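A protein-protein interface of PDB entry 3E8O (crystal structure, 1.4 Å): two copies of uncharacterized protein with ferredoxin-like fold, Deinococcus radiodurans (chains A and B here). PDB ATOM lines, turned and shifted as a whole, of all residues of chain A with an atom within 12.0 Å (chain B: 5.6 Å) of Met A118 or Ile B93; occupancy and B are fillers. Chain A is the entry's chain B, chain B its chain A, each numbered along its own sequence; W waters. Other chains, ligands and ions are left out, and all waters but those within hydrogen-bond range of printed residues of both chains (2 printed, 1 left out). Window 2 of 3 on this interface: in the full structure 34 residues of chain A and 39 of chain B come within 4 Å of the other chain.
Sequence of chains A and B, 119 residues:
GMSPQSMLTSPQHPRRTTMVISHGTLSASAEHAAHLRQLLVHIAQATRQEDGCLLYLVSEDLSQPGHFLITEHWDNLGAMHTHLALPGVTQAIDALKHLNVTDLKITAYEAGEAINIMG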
ATOM      1  N   ALA A 114      -8.778  -3.466 -16.114  1.00  0.00           N
ATOM      2  CA  ALA A 114      -9.134  -4.640 -16.925  1.00  0.00           C
ATOM      3  C   ALA A 114     -10.369  -4.388 -17.762  1.00  0.00           C
ATOM      4  O   ALA A 114     -11.350  -3.851 -17.283  1.00  0.00           O
ATOM      5  CB  ALA A 114      -9.372  -5.885 -16.041  1.00  0.00           C
ATOM      6  N   ILE A 115     -10.262  -4.802 -19.015  1.00  0.00           N
ATOM      7  CA  ILE A 115     -11.350  -4.809 -19.968  1.00  0.00           C
ATOM      8  C   ILE A 115     -11.624  -6.266 -20.357  1.00  0.00           C
ATOM      9  O   ILE A 115     -10.810  -6.901 -21.046  1.00  0.00           O
ATOM     10  CB  ILE A 115     -11.058  -3.943 -21.237  1.00  0.00           C
ATOM     11  CG1 ILE A 115     -10.564  -2.561 -20.873  1.00  0.00           C
ATOM     12  CG2 ILE A 115     -12.236  -3.949 -22.184  1.00  0.00           C
ATOM     13  CD1 ILE A 115      -9.887  -1.809 -22.029  1.00  0.00           C
ATOM     14  N   ASN A 116     -12.720  -6.834 -19.859  1.00  0.00           N
ATOM     15  CA  ASN A 116     -13.073  -8.229 -20.187  1.00  0.00           C
ATOM     16  C   ASN A 116     -13.512  -8.346 -21.619  1.00  0.00           C
ATOM     17  O   ASN A 116     -14.434  -7.629 -22.061  1.00  0.00           O
ATOM     18  CB  ASN A 116     -14.106  -8.772 -19.239  1.00  0.00           C
ATOM     19  CG  ASN A 116     -13.549  -8.993 -17.888  1.00  0.00           C
ATOM     20  OD1 ASN A 116     -12.452  -9.495 -17.783  1.00  0.00           O
ATOM     21  ND2 ASN A 116     -14.270  -8.645 -16.853  1.00  0.00           N
ATOM     22  N   ILE A 117     -12.838  -9.237 -22.340  1.00  0.00           N
ATOM     23  CA  ILE A 117     -13.092  -9.442 -23.784  1.00  0.00           C
ATOM     24  C   ILE A 117     -13.947 -10.680 -24.024  1.00  0.00           C
ATOM     25  O   ILE A 117     -15.022 -10.606 -24.614  1.00  0.00           O
ATOM     26  CB  ILE A 117     -11.797  -9.518 -24.553  1.00  0.00           C
ATOM     27  CG1 ILE A 117     -11.031  -8.196 -24.369  1.00  0.00           C
ATOM     28  CG2 ILE A 117     -12.018  -9.851 -26.057  1.00  0.00           C
ATOM     29  CD1 ILE A 117     -11.796  -6.940 -24.837  1.00  0.00           C
ATOM     30  N   MET A 118     -13.467 -11.822 -23.548  1.00  0.00           N
ATOM     31  CA  MET A 118     -14.289 -13.042 -23.575  1.00  0.00           C
ATOM     32  C   MET A 118     -13.749 -14.072 -22.627  1.00  0.00           C
ATOM     33  O   MET A 118     -12.617 -13.996 -22.156  1.00  0.00           O
ATOM     34  CB  MET A 118     -14.450 -13.629 -24.978  1.00  0.00           C
ATOM     35  CG  MET A 118     -13.133 -14.232 -25.560  1.00  0.00           C
ATOM     36  SD  MET A 118     -13.116 -14.729 -27.372  1.00  0.00           S
ATOM     37  CE  MET A 118     -13.266 -12.990 -28.279  1.00  0.00           C
ATOM     38  N   GLY A 119     -14.639 -14.994 -22.295  1.00  0.00           N
ATOM     39  CA  GLY A 119     -14.328 -16.046 -21.337  1.00  0.00           C
ATOM     40  C   GLY A 119     -14.248 -15.623 -19.911  1.00  0.00           C
ATOM     41  O   GLY A 119     -14.516 -14.452 -19.624  1.00  0.00           O
ATOM     42  OXT GLY A 119     -13.930 -16.509 -19.122  1.00  0.00           O
ATOM     43  N   LEU B  84     -12.724  -7.827 -33.147  1.00  0.00           N
ATOM     44  CA  LEU B  84     -13.546  -8.747 -32.369  1.00  0.00           C
ATOM     45  C   LEU B  84     -14.883  -9.079 -33.036  1.00  0.00           C
ATOM     46  O   LEU B  84     -15.451 -10.136 -32.827  1.00  0.00           O
ATOM     47  CB  LEU B  84     -13.760  -8.197 -30.973  1.00  0.00           C
ATOM     48  CG  LEU B  84     -12.469  -8.319 -30.132  1.00  0.00           C
ATOM     49  CD1 LEU B  84     -12.565  -7.417 -28.922  1.00  0.00           C
ATOM     50  CD2 LEU B  84     -12.213  -9.798 -29.728  1.00  0.00           C
ATOM     51  N   GLY B  88     -14.449 -13.841 -39.196  1.00  0.00           N
ATOM     52  CA  GLY B  88     -13.337 -14.780 -39.012  1.00  0.00           C
ATOM     53  C   GLY B  88     -13.078 -15.111 -37.549  1.00  0.00           C
ATOM     54  O   GLY B  88     -12.639 -16.228 -37.229  1.00  0.00           O
ATOM     55  N   VAL B  89     -13.407 -14.155 -36.678  1.00  0.00           N
ATOM     56  CA  VAL B  89     -13.246 -14.331 -35.213  1.00  0.00           C
ATOM     57  C   VAL B  89     -14.357 -15.253 -34.727  1.00  0.00           C
ATOM     58  O   VAL B  89     -14.116 -16.180 -33.945  1.00  0.00           O
ATOM     59  CB  VAL B  89     -13.209 -12.975 -34.450  1.00  0.00           C
ATOM     60  CG1 VAL B  89     -13.458 -13.145 -32.943  1.00  0.00           C
ATOM     61  CG2 VAL B  89     -11.862 -12.349 -34.703  1.00  0.00           C
ATOM     62  N   THR B  90     -15.567 -15.022 -35.218  1.00  0.00           N
ATOM     63  CA  THR B  90     -16.706 -15.894 -34.875  1.00  0.00           C
ATOM     64  C   THR B  90     -16.400 -17.327 -35.271  1.00  0.00           C
ATOM     65  O   THR B  90     -16.613 -18.268 -34.507  1.00  0.00           O
ATOM     66  CB  THR B  90     -18.003 -15.455 -35.584  1.00  0.00           C
ATOM     67  OG1 THR B  90     -18.385 -14.201 -35.032  1.00  0.00           O
ATOM     68  CG2 THR B  90     -19.142 -16.469 -35.384  1.00  0.00           C
ATOM     69  N   GLN B  91     -15.842 -17.468 -36.473  1.00  0.00           N
ATOM     70  CA  GLN B  91     -15.522 -18.765 -37.025  1.00  0.00           C
ATOM     71  C   GLN B  91     -14.460 -19.456 -36.190  1.00  0.00           C
ATOM     72  O   GLN B  91     -14.546 -20.630 -35.915  1.00  0.00           O
ATOM     73  CB  GLN B  91     -15.025 -18.635 -38.457  1.00  0.00           C
ATOM     74  CG  GLN B  91     -16.044 -18.074 -39.460  1.00  0.00           C
ATOM     75  CD  GLN B  91     -15.347 -17.701 -40.769  1.00  0.00           C
ATOM     76  OE1 GLN B  91     -14.278 -18.229 -41.080  1.00  0.00           O
ATOM     77  NE2 GLN B  91     -15.900 -16.749 -41.487  1.00  0.00           N
ATOM     78  N   ALA B  92     -13.485 -18.688 -35.722  1.00  0.00           N
ATOM     79  CA  ALA B  92     -12.399 -19.255 -34.909  1.00  0.00           C
ATOM     80  C   ALA B  92     -12.934 -19.727 -33.566  1.00  0.00           C
ATOM     81  O   ALA B  92     -12.568 -20.787 -33.058  1.00  0.00           O
ATOM     82  CB  ALA B  92     -11.279 -18.210 -34.703  1.00  0.00           C
ATOM     83  N   ILE B  93     -13.814 -18.934 -32.967  1.00  0.00           N
ATOM     84  CA  ILE B  93     -14.437 -19.309 -31.694  1.00  0.00           C
ATOM     85  C   ILE B  93     -15.235 -20.576 -31.855  1.00  0.00           C
ATOM     86  O   ILE B  93     -15.199 -21.497 -31.015  1.00  0.00           O
ATOM     87  CB  ILE B  93     -15.301 -18.157 -31.126  1.00  0.00           C
ATOM     88  CG1 ILE B  93     -14.352 -17.022 -30.719  1.00  0.00           C
ATOM     89  CG2 ILE B  93     -16.199 -18.678 -30.030  1.00  0.00           C
ATOM     90  CD1 ILE B  93     -15.010 -15.690 -30.454  1.00  0.00           C
ATOM     91  N   ASP B  94     -15.913 -20.668 -32.980  1.00  0.00           N
ATOM     92  CA  ASP B  94     -16.727 -21.859 -33.257  1.00  0.00           C
ATOM     93  C   ASP B  94     -15.848 -23.105 -33.374  1.00  0.00           C
ATOM     94  O   ASP B  94     -16.170 -24.201 -32.861  1.00  0.00           O
ATOM     95  CB  ASP B  94     -17.594 -21.660 -34.504  1.00  0.00           C
ATOM     96  CG  ASP B  94     -18.837 -20.827 -34.198  1.00  0.00           C
ATOM     97  OD1 ASP B  94     -19.203 -20.739 -32.998  1.00  0.00           O
ATOM     98  OD2 ASP B  94     -19.457 -20.277 -35.142  1.00  0.00           O
ATOM     99  N   ALA B  95     -14.717 -22.924 -34.021  1.00  0.00           N
ATOM    100  CA  ALA B  95     -13.759 -24.021 -34.205  1.00  0.00           C
ATOM    101  C   ALA B  95     -13.267 -24.560 -32.852  1.00  0.00           C
ATOM    102  O   ALA B  95     -13.029 -25.786 -32.668  1.00  0.00           O
ATOM    103  CB  ALA B  95     -12.594 -23.594 -35.148  1.00  0.00           C
ATOM    104  N   LEU B  96     -13.109 -23.658 -31.897  1.00  0.00           N
ATOM    105  CA  LEU B  96     -12.657 -24.052 -30.557  1.00  0.00           C
ATOM    106  C   LEU B  96     -13.642 -24.991 -29.890  1.00  0.00           C
ATOM    107  O   LEU B  96     -13.268 -25.949 -29.196  1.00  0.00           O
ATOM    108  CB  LEU B  96     -12.420 -22.839 -29.651  1.00  0.00           C
ATOM    109  CG  LEU B  96     -11.276 -21.913 -30.026  1.00  0.00           C
ATOM    110  CD1 LEU B  96     -11.277 -20.661 -29.105  1.00  0.00           C
ATOM    111  CD2 LEU B  96      -9.915 -22.597 -29.997  1.00  0.00           C
ATOM    112  N   LYS B  97     -14.918 -24.737 -30.140  1.00  0.00           N
ATOM    113  CA  LYS B  97     -15.991 -25.553 -29.545  1.00  0.00           C
ATOM    114  C   LYS B  97     -15.796 -26.976 -29.958  1.00  0.00           C
ATOM    115  O   LYS B  97     -15.976 -27.930 -29.192  1.00  0.00           O
ATOM    116  CB  LYS B  97     -17.414 -25.079 -29.954  1.00  0.00           C
ATOM    117  CG  LYS B  97     -17.915 -23.857 -29.210  1.00  0.00           C
ATOM    118  CD  LYS B  97     -19.436 -23.520 -29.473  1.00  0.00           C
ATOM    119  CE  LYS B  97     -19.751 -23.204 -30.922  1.00  0.00           C
ATOM    120  NZ  LYS B  97     -21.178 -22.710 -31.163  1.00  0.00           N
ATOM    121  N   LEU B 104     -10.878 -20.555 -23.060  1.00  0.00           N
ATOM    122  CA  LEU B 104     -10.303 -19.311 -23.548  1.00  0.00           C
ATOM    123  C   LEU B 104     -10.779 -18.127 -22.727  1.00  0.00           C
ATOM    124  O   LEU B 104     -11.970 -17.906 -22.562  1.00  0.00           O
ATOM    125  CB  LEU B 104     -10.707 -19.072 -25.014  1.00  0.00           C
ATOM    126  CG  LEU B 104     -10.289 -17.749 -25.685  1.00  0.00           C
ATOM    127  CD1 LEU B 104      -8.797 -17.514 -25.713  1.00  0.00           C
ATOM    128  CD2 LEU B 104     -10.881 -17.589 -27.101  1.00  0.00           C
ATOM    129  N   LYS B 105      -9.838 -17.334 -22.235  1.00  0.00           N
ATOM    130  CA  LYS B 105     -10.119 -16.103 -21.513  1.00  0.00           C
ATOM    131  C   LYS B 105      -9.199 -15.019 -22.012  1.00  0.00           C
ATOM    132  O   LYS B 105      -7.994 -15.217 -22.071  1.00  0.00           O
ATOM    133  CB  LYS B 105      -9.991 -16.252 -19.989  1.00  0.00           C
ATOM    134  CG  LYS B 105     -10.452 -15.009 -19.216  1.00  0.00           C
ATOM    135  CD  LYS B 105     -10.400 -15.130 -17.768  1.00  0.00           C
ATOM    136  CE  LYS B 105     -10.769 -13.826 -17.080  1.00  0.00           C
ATOM    137  NZ  LYS B 105     -12.204 -13.452 -17.294  1.00  0.00           N
ATOM    138  N   ILE B 106      -9.798 -13.900 -22.368  1.00  0.00           N
ATOM    139  CA  ILE B 106      -9.029 -12.744 -22.856  1.00  0.00           C
ATOM    140  C   ILE B 106      -9.415 -11.500 -22.087  1.00  0.00           C
ATOM    141  O   ILE B 106     -10.596 -11.231 -21.878  1.00  0.00           O
ATOM    142  CB  ILE B 106      -9.297 -12.504 -24.365  1.00  0.00           C
ATOM    143  CG1 ILE B 106      -8.978 -13.734 -25.239  1.00  0.00           C
ATOM    144  CG2 ILE B 106      -8.505 -11.289 -24.901  1.00  0.00           C
ATOM    145  CD1 ILE B 106      -9.331 -13.541 -26.737  1.00  0.00           C
ATOM    146  N   THR B 107      -8.389 -10.812 -21.620  1.00  0.00           N
ATOM    147  CA  THR B 107      -8.536  -9.520 -20.899  1.00  0.00           C
ATOM    148  C   THR B 107      -7.599  -8.531 -21.586  1.00  0.00           C
ATOM    149  O   THR B 107      -6.501  -8.880 -21.931  1.00  0.00           O
ATOM    150  CB  THR B 107      -8.193  -9.665 -19.391  1.00  0.00           C
ATOM    151  OG1 THR B 107      -8.872 -10.820 -18.881  1.00  0.00           O
ATOM    152  CG2 THR B 107      -8.570  -8.363 -18.621  1.00  0.00           C
HETATM  153  O   HOH W   1     -13.695 -15.697 -16.568  1.00  0.00           O
HETATM  154  O   HOH W   2     -10.451 -10.535 -16.459  1.00  0.00           O
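The backbone carbonyl oxygen (O) of Met A118 is in hydrogen-bond range of the backbone NH (N) of Ile B106 (2.8 Å).
O of Gly A119 is in salt-bridge range of NZ of Lys B105, at 3.4 Å.
The backbone carbonyl oxygen of Ile B106 sits at hydrogen-bond distance from the backbone NH of Ile A117 (3.0 Å).
Among the printed residues, pairs that only touch across the chains: Gly A119 with Leu B104 (3.2 Å), Met A118 with Lys B105 (3.3 Å), Ile A115 with Thr B107 (3.5 Å), Met A118 with Leu B104 (3.6 Å), Met A118 with Leu B84 (3.7 Å), Ala A114 with Thr B107 (3.7 Å), Ile A117 with Leu B84 (3.7 Å), Met A118 with Ile B93 (3.7 Å), Asn A116 with Thr B107 (3.97 Å) and Asn A116 with Lys B105 (3.99 Å).
Printed residues of chain B within 4 Å of Met A118: Leu B84 (3.7 Å), Ile B93 (3.7 Å), Leu B104 (3.6 Å), Lys B105 (3.3 Å) and Ile B106 (2.8 Å).
Of the printed residues of chain A, Ile B93 touches Met A118.
No residue of chain A comes within 4 Å of Val B89.
No residue of chain A comes within 4 Å of Thr B90.
No residue of chain A comes within 4 Å of Ala B95.
No residue of chain A comes within 4 Å of Lys B97.
Of the printed residues of chain A, Thr B107 touches Ala A114, Ile A115 and Asn A116.
Printed residues of chain B within 4 Å of Gly A119: Leu B104 (3.2 Å) and Lys B105 (3.4 Å).
Of the printed residues of chain A, Leu B84 touches Ile A117 and Met A118.
The nearest printed residue of chain B that does not touch Met A118 is Val B89 (4.7 Å).
The nearest printed residue of chain A that does not touch Ile B93 is Ile A117 (7.7 Å).
The nearest printed residue of chain B that does not touch Asn A116 is Ile B106 (4.1 Å).
Hydrophobic or aromatic side chains of chain B within 4 Å of the printed part of chain A: Leu B84, Ile B93, Leu B104 and Ile B106.
No position is printed for both chains.
Of the 13 pairs that touch across the chains among the printed residues, none has its exchanged pair printed and touching as well.
Water W2 bridges OD1 of Asn A116 and OG1 of Thr B107.
Water W1 lies within hydrogen-bond range of the chain-end carboxylate of Gly A119 (2.7 Å) and the side-chain amino group of Lys B105 (2.8 Å).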
